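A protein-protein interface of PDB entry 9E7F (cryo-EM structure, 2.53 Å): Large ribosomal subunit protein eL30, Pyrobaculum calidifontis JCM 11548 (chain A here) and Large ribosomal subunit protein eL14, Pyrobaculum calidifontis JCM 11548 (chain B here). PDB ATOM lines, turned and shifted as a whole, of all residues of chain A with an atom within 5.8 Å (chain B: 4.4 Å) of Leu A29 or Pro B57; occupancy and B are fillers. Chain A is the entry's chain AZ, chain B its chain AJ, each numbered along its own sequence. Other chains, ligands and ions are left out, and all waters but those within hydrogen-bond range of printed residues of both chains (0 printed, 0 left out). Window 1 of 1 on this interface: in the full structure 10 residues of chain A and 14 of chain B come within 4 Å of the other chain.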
ATOM      1  N   THR A  24       0.456   7.056  13.463  1.00  0.00           N
ATOM      2  CA  THR A  24       1.247   8.277  13.557  1.00  0.00           C
ATOM      3  C   THR A  24       1.626   8.584  14.998  1.00  0.00           C
ATOM      4  O   THR A  24       2.760   8.990  15.275  1.00  0.00           O
ATOM      5  CB  THR A  24       0.469   9.443  12.957  1.00  0.00           C
ATOM      6  OG1 THR A  24       0.159   9.155  11.590  1.00  0.00           O
ATOM      7  CG2 THR A  24       1.292  10.711  13.023  1.00  0.00           C
ATOM      8  N   LYS A  25       0.687   8.409  15.927  1.00  0.00           N
ATOM      9  CA  LYS A  25       0.999   8.622  17.334  1.00  0.00           C
ATOM     10  C   LYS A  25       2.019   7.607  17.824  1.00  0.00           C
ATOM     11  O   LYS A  25       2.915   7.942  18.606  1.00  0.00           O
ATOM     12  CB  LYS A  25      -0.276   8.554  18.170  1.00  0.00           C
ATOM     13  CG  LYS A  25      -0.938   9.898  18.396  1.00  0.00           C
ATOM     14  CD  LYS A  25      -2.439   9.752  18.552  1.00  0.00           C
ATOM     15  CE  LYS A  25      -2.820   8.326  18.905  1.00  0.00           C
ATOM     16  NZ  LYS A  25      -4.282   8.087  18.763  1.00  0.00           N
ATOM     17  N   LYS A  26       1.895   6.357  17.381  1.00  0.00           N
ATOM     18  CA  LYS A  26       2.909   5.360  17.693  1.00  0.00           C
ATOM     19  C   LYS A  26       4.245   5.716  17.056  1.00  0.00           C
ATOM     20  O   LYS A  26       5.297   5.591  17.690  1.00  0.00           O
ATOM     21  CB  LYS A  26       2.447   3.982  17.225  1.00  0.00           C
ATOM     22  CG  LYS A  26       1.946   3.076  18.330  1.00  0.00           C
ATOM     23  CD  LYS A  26       3.099   2.428  19.077  1.00  0.00           C
ATOM     24  CE  LYS A  26       2.714   1.054  19.606  1.00  0.00           C
ATOM     25  NZ  LYS A  26       1.384   1.049  20.274  1.00  0.00           N
ATOM     26  N   SER A  27       4.226   6.160  15.798  1.00  0.00           N
ATOM     27  CA  SER A  27       5.470   6.511  15.127  1.00  0.00           C
ATOM     28  C   SER A  27       6.069   7.797  15.663  1.00  0.00           C
ATOM     29  O   SER A  27       7.290   7.957  15.621  1.00  0.00           O
ATOM     30  CB  SER A  27       5.260   6.634  13.625  1.00  0.00           C
ATOM     31  OG  SER A  27       6.464   6.330  12.948  1.00  0.00           O
ATOM     32  N   LEU A  28       5.245   8.721  16.148  1.00  0.00           N
ATOM     33  CA  LEU A  28       5.779   9.880  16.848  1.00  0.00           C
ATOM     34  C   LEU A  28       6.319   9.496  18.221  1.00  0.00           C
ATOM     35  O   LEU A  28       7.399   9.945  18.618  1.00  0.00           O
ATOM     36  CB  LEU A  28       4.696  10.943  16.984  1.00  0.00           C
ATOM     37  CG  LEU A  28       5.201  12.376  16.972  1.00  0.00           C
ATOM     38  CD1 LEU A  28       6.532  12.445  16.257  1.00  0.00           C
ATOM     39  CD2 LEU A  28       4.180  13.266  16.310  1.00  0.00           C
ATOM     40  N   LEU A  29       5.583   8.666  18.957  1.00  0.00           N
ATOM     41  CA  LEU A  29       5.946   8.365  20.336  1.00  0.00           C
ATOM     42  C   LEU A  29       7.139   7.421  20.417  1.00  0.00           C
ATOM     43  O   LEU A  29       8.048   7.636  21.224  1.00  0.00           O
ATOM     44  CB  LEU A  29       4.745   7.765  21.067  1.00  0.00           C
ATOM     45  CG  LEU A  29       4.326   8.379  22.403  1.00  0.00           C
ATOM     46  CD1 LEU A  29       4.482   9.886  22.389  1.00  0.00           C
ATOM     47  CD2 LEU A  29       2.895   8.000  22.727  1.00  0.00           C
ATOM     48  N   THR A  30       7.159   6.381  19.585  1.00  0.00           N
ATOM     49  CA  THR A  30       8.146   5.319  19.699  1.00  0.00           C
ATOM     50  C   THR A  30       9.151   5.282  18.559  1.00  0.00           C
ATOM     51  O   THR A  30      10.259   4.775  18.754  1.00  0.00           O
ATOM     52  CB  THR A  30       7.445   3.957  19.775  1.00  0.00           C
ATOM     53  OG1 THR A  30       6.339   4.043  20.680  1.00  0.00           O
ATOM     54  CG2 THR A  30       8.404   2.889  20.260  1.00  0.00           C
ATOM     55  N   GLY A  31       8.793   5.792  17.380  1.00  0.00           N
ATOM     56  CA  GLY A  31       9.694   5.848  16.252  1.00  0.00           C
ATOM     57  C   GLY A  31      10.329   7.216  16.090  1.00  0.00           C
ATOM     58  O   GLY A  31      10.267   8.080  16.968  1.00  0.00           O
ATOM     59  N   TYR A  52       1.435  18.044  20.504  1.00  0.00           N
ATOM     60  CA  TYR A  52       2.136  17.873  21.769  1.00  0.00           C
ATOM     61  C   TYR A  52       3.199  16.787  21.659  1.00  0.00           C
ATOM     62  O   TYR A  52       4.330  16.967  22.118  1.00  0.00           O
ATOM     63  CB  TYR A  52       1.126  17.586  22.889  1.00  0.00           C
ATOM     64  CG  TYR A  52       1.709  17.193  24.236  1.00  0.00           C
ATOM     65  CD1 TYR A  52       1.952  15.866  24.571  1.00  0.00           C
ATOM     66  CD2 TYR A  52       2.055  18.165  25.155  1.00  0.00           C
ATOM     67  CE1 TYR A  52       2.488  15.526  25.782  1.00  0.00           C
ATOM     68  CE2 TYR A  52       2.601  17.835  26.367  1.00  0.00           C
ATOM     69  CZ  TYR A  52       2.814  16.517  26.679  1.00  0.00           C
ATOM     70  OH  TYR A  52       3.355  16.191  27.901  1.00  0.00           O
ATOM     71  N   TYR A  53       2.858  15.653  21.048  1.00  0.00           N
ATOM     72  CA  TYR A  53       3.854  14.604  20.860  1.00  0.00           C
ATOM     73  C   TYR A  53       4.907  15.037  19.851  1.00  0.00           C
ATOM     74  O   TYR A  53       6.087  14.697  19.991  1.00  0.00           O
ATOM     75  CB  TYR A  53       3.183  13.308  20.404  1.00  0.00           C
ATOM     76  CG  TYR A  53       2.211  12.726  21.402  1.00  0.00           C
ATOM     77  CD1 TYR A  53       2.319  13.006  22.751  1.00  0.00           C
ATOM     78  CD2 TYR A  53       1.175  11.899  20.988  1.00  0.00           C
ATOM     79  CE1 TYR A  53       1.432  12.489  23.660  1.00  0.00           C
ATOM     80  CE2 TYR A  53       0.280  11.373  21.895  1.00  0.00           C
ATOM     81  CZ  TYR A  53       0.416  11.672  23.232  1.00  0.00           C
ATOM     82  OH  TYR A  53      -0.464  11.154  24.154  1.00  0.00           O
ATOM     83  N   LEU A  56       7.223  17.486  21.652  1.00  0.00           N
ATOM     84  CA  LEU A  56       8.166  16.715  22.450  1.00  0.00           C
ATOM     85  C   LEU A  56       9.173  15.997  21.564  1.00  0.00           C
ATOM     86  O   LEU A  56      10.376  16.001  21.840  1.00  0.00           O
ATOM     87  CB  LEU A  56       7.415  15.714  23.324  1.00  0.00           C
ATOM     88  CG  LEU A  56       6.920  16.137  24.702  1.00  0.00           C
ATOM     89  CD1 LEU A  56       6.455  17.575  24.723  1.00  0.00           C
ATOM     90  CD2 LEU A  56       5.799  15.215  25.113  1.00  0.00           C
ATOM     91  N   LYS B   3      12.611   9.831  19.590  1.00  0.00           N
ATOM     92  CA  LYS B   3      11.505   9.117  20.212  1.00  0.00           C
ATOM     93  C   LYS B   3      11.191   9.690  21.594  1.00  0.00           C
ATOM     94  O   LYS B   3      12.090   9.995  22.378  1.00  0.00           O
ATOM     95  CB  LYS B   3      11.825   7.620  20.291  1.00  0.00           C
ATOM     96  CG  LYS B   3      12.536   7.161  21.562  1.00  0.00           C
ATOM     97  CD  LYS B   3      13.185   5.801  21.361  1.00  0.00           C
ATOM     98  CE  LYS B   3      12.137   4.708  21.288  1.00  0.00           C
ATOM     99  NZ  LYS B   3      10.976   5.028  22.154  1.00  0.00           N
ATOM    100  N   VAL B   4       9.900   9.856  21.882  1.00  0.00           N
ATOM    101  CA  VAL B   4       9.502  10.479  23.141  1.00  0.00           C
ATOM    102  C   VAL B   4       9.468   9.448  24.258  1.00  0.00           C
ATOM    103  O   VAL B   4      10.006   9.672  25.348  1.00  0.00           O
ATOM    104  CB  VAL B   4       8.146  11.187  22.984  1.00  0.00           C
ATOM    105  CG1 VAL B   4       7.333  11.069  24.252  1.00  0.00           C
ATOM    106  CG2 VAL B   4       8.363  12.633  22.646  1.00  0.00           C
ATOM    107  N   ILE B   5       8.842   8.303  24.007  1.00  0.00           N
ATOM    108  CA  ILE B   5       8.744   7.258  25.015  1.00  0.00           C
ATOM    109  C   ILE B   5      10.063   6.509  25.014  1.00  0.00           C
ATOM    110  O   ILE B   5      10.248   5.543  24.270  1.00  0.00           O
ATOM    111  CB  ILE B   5       7.551   6.324  24.754  1.00  0.00           C
ATOM    112  CG1 ILE B   5       6.247   7.115  24.815  1.00  0.00           C
ATOM    113  CG2 ILE B   5       7.514   5.218  25.773  1.00  0.00           C
ATOM    114  CD1 ILE B   5       6.138   8.020  26.015  1.00  0.00           C
ATOM    115  N   ARG B   9      12.106   8.780  30.904  1.00  0.00           N
ATOM    116  CA  ARG B   9      11.022   9.719  30.657  1.00  0.00           C
ATOM    117  C   ARG B   9       9.944   9.552  31.718  1.00  0.00           C
ATOM    118  O   ARG B   9       9.488   8.436  31.978  1.00  0.00           O
ATOM    119  CB  ARG B   9      10.432   9.511  29.261  1.00  0.00           C
ATOM    120  CG  ARG B   9       9.150  10.282  28.980  1.00  0.00           C
ATOM    121  CD  ARG B   9       9.273  11.747  29.350  1.00  0.00           C
ATOM    122  NE  ARG B   9      10.213  12.461  28.497  1.00  0.00           N
ATOM    123  CZ  ARG B   9       9.865  13.203  27.456  1.00  0.00           C
ATOM    124  NH1 ARG B   9       8.599  13.353  27.110  1.00  0.00           N
ATOM    125  NH2 ARG B   9      10.810  13.817  26.754  1.00  0.00           N
ATOM    126  N   VAL B  10       9.545  10.664  32.322  1.00  0.00           N
ATOM    127  CA  VAL B  10       8.442  10.669  33.272  1.00  0.00           C
ATOM    128  C   VAL B  10       7.132  10.563  32.505  1.00  0.00           C
ATOM    129  O   VAL B  10       6.885  11.324  31.563  1.00  0.00           O
ATOM    130  CB  VAL B  10       8.480  11.935  34.138  1.00  0.00           C
ATOM    131  CG1 VAL B  10       7.275  11.986  35.049  1.00  0.00           C
ATOM    132  CG2 VAL B  10       9.758  11.982  34.938  1.00  0.00           C
ATOM    133  N   VAL B  11       6.292   9.614  32.900  1.00  0.00           N
ATOM    134  CA  VAL B  11       5.032   9.347  32.225  1.00  0.00           C
ATOM    135  C   VAL B  11       3.921   9.312  33.260  1.00  0.00           C
ATOM    136  O   VAL B  11       4.132   8.920  34.412  1.00  0.00           O
ATOM    137  CB  VAL B  11       5.078   8.021  31.444  1.00  0.00           C
ATOM    138  CG1 VAL B  11       6.295   7.978  30.559  1.00  0.00           C
ATOM    139  CG2 VAL B  11       5.090   6.852  32.405  1.00  0.00           C
ATOM    140  N   ILE B  55      -0.179   5.358  28.754  1.00  0.00           N
ATOM    141  CA  ILE B  55       0.632   6.325  29.474  1.00  0.00           C
ATOM    142  C   ILE B  55       0.647   7.613  28.675  1.00  0.00           C
ATOM    143  O   ILE B  55       0.494   7.606  27.450  1.00  0.00           O
ATOM    144  CB  ILE B  55       2.069   5.824  29.701  1.00  0.00           C
ATOM    145  CG1 ILE B  55       2.742   5.547  28.359  1.00  0.00           C
ATOM    146  CG2 ILE B  55       2.066   4.588  30.573  1.00  0.00           C
ATOM    147  CD1 ILE B  55       4.239   5.580  28.414  1.00  0.00           C
ATOM    148  N   GLU B  56       0.828   8.726  29.374  1.00  0.00           N
ATOM    149  CA  GLU B  56       0.987  10.017  28.727  1.00  0.00           C
ATOM    150  C   GLU B  56       2.371  10.552  29.053  1.00  0.00           C
ATOM    151  O   GLU B  56       2.678  10.770  30.237  1.00  0.00           O
ATOM    152  CB  GLU B  56      -0.083  11.009  29.173  1.00  0.00           C
ATOM    153  CG  GLU B  56       0.050  12.374  28.517  1.00  0.00           C
ATOM    154  CD  GLU B  56      -0.500  12.401  27.104  1.00  0.00           C
ATOM    155  OE1 GLU B  56      -0.753  11.319  26.539  1.00  0.00           O
ATOM    156  OE2 GLU B  56      -0.677  13.507  26.556  1.00  0.00           O
ATOM    157  N   PRO B  57       3.236  10.755  28.067  1.00  0.00           N
ATOM    158  CA  PRO B  57       4.550  11.327  28.355  1.00  0.00           C
ATOM    159  C   PRO B  57       4.431  12.766  28.816  1.00  0.00           C
ATOM    160  O   PRO B  57       3.555  13.514  28.380  1.00  0.00           O
ATOM    161  CB  PRO B  57       5.276  11.237  27.012  1.00  0.00           C
ATOM    162  CG  PRO B  57       4.189  11.305  26.017  1.00  0.00           C
ATOM    163  CD  PRO B  57       3.019  10.583  26.624  1.00  0.00           C
ATOM    164  N   THR B  58       5.324  13.146  29.711  1.00  0.00           N
ATOM    165  CA  THR B  58       5.458  14.528  30.130  1.00  0.00           C
ATOM    166  C   THR B  58       6.675  15.146  29.450  1.00  0.00           C
ATOM    167  O   THR B  58       7.452  14.470  28.776  1.00  0.00           O
ATOM    168  CB  THR B  58       5.573  14.620  31.654  1.00  0.00           C
ATOM    169  OG1 THR B  58       5.246  15.946  32.081  1.00  0.00           O
ATOM    170  CG2 THR B  58       6.975  14.288  32.096  1.00  0.00           C
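The backbone carbonyl oxygen (O) of Thr A30 lies close to the side-chain amino group (NZ) of Lys B3 (3.5 Å).
The backbone NH of Val B4 sits at hydrogen-bond distance from the backbone carbonyl oxygen of Leu A29 (3.0 Å).
The backbone NH of Ile B5 sits at hydrogen-bond distance from the backbone carbonyl oxygen of Leu A29, at 3.0 Å.
The side-chain carboxylate (OE1) of Glu B56 is in hydrogen-bond range of the side-chain hydroxyl (OH) of Tyr A53 (2.4 Å).
The side-chain hydroxyl (OH) of Tyr A52 sits at hydrogen-bond distance from the backbone carbonyl oxygen (O) of Pro B57 (2.7 Å).
O of Thr B58 sits close to NE of Arg B9, at 3.4 Å.
The backbone NH (N) of Thr B58 sits close to the backbone carbonyl oxygen (O) of Val B10, 3.0 Å away.
Among the printed residues, pairs that only touch across the chains: Leu A29 with Lys B3 (3.8 Å), Leu A29 with Pro B57 (3.9 Å), Gly A31 with Lys B3 (3.6 Å), Tyr A52 with Glu B56 (3.8 Å), Tyr A52 with Thr B58 (3.5 Å), Tyr A53 with Pro B57 (3.8 Å), Leu A56 with Val B4 (3.3 Å) and Leu A56 with Arg B9 (3.9 Å).
Leu A29 touches just these residues of chain B: Lys B3, Val B4, Ile B5 and Pro B57.
Printed residues of chain B within 4 Å of Leu A56: Val B4 and Arg B9.
Of the printed residues of chain A, Val B4 touches Leu A29 and Leu A56.
Of the printed residues of chain A, Arg B9 touches Leu A56.
Val B11 touches none of the printed residues of chain A.
The nearest printed residue of chain B that does not touch Leu A29 is Ile B55 (5.3 Å).
Of the 11 printed residues of chain A, 6 touch a printed residue of chain B.
Hydrophobic or aromatic side chains of chain A that line the printed part of chain B: Leu A29, Tyr A52, Tyr A53 and Leu A56.
Hydrophobic or aromatic side chains of chain B within 4 Å of the printed part of chain A: Val B4, Ile B5 and Pro B57.
Among the printed residues, no Asp or Glu carboxylate lies within 4 Å of a Lys or Arg side-chain nitrogen of the other chain.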
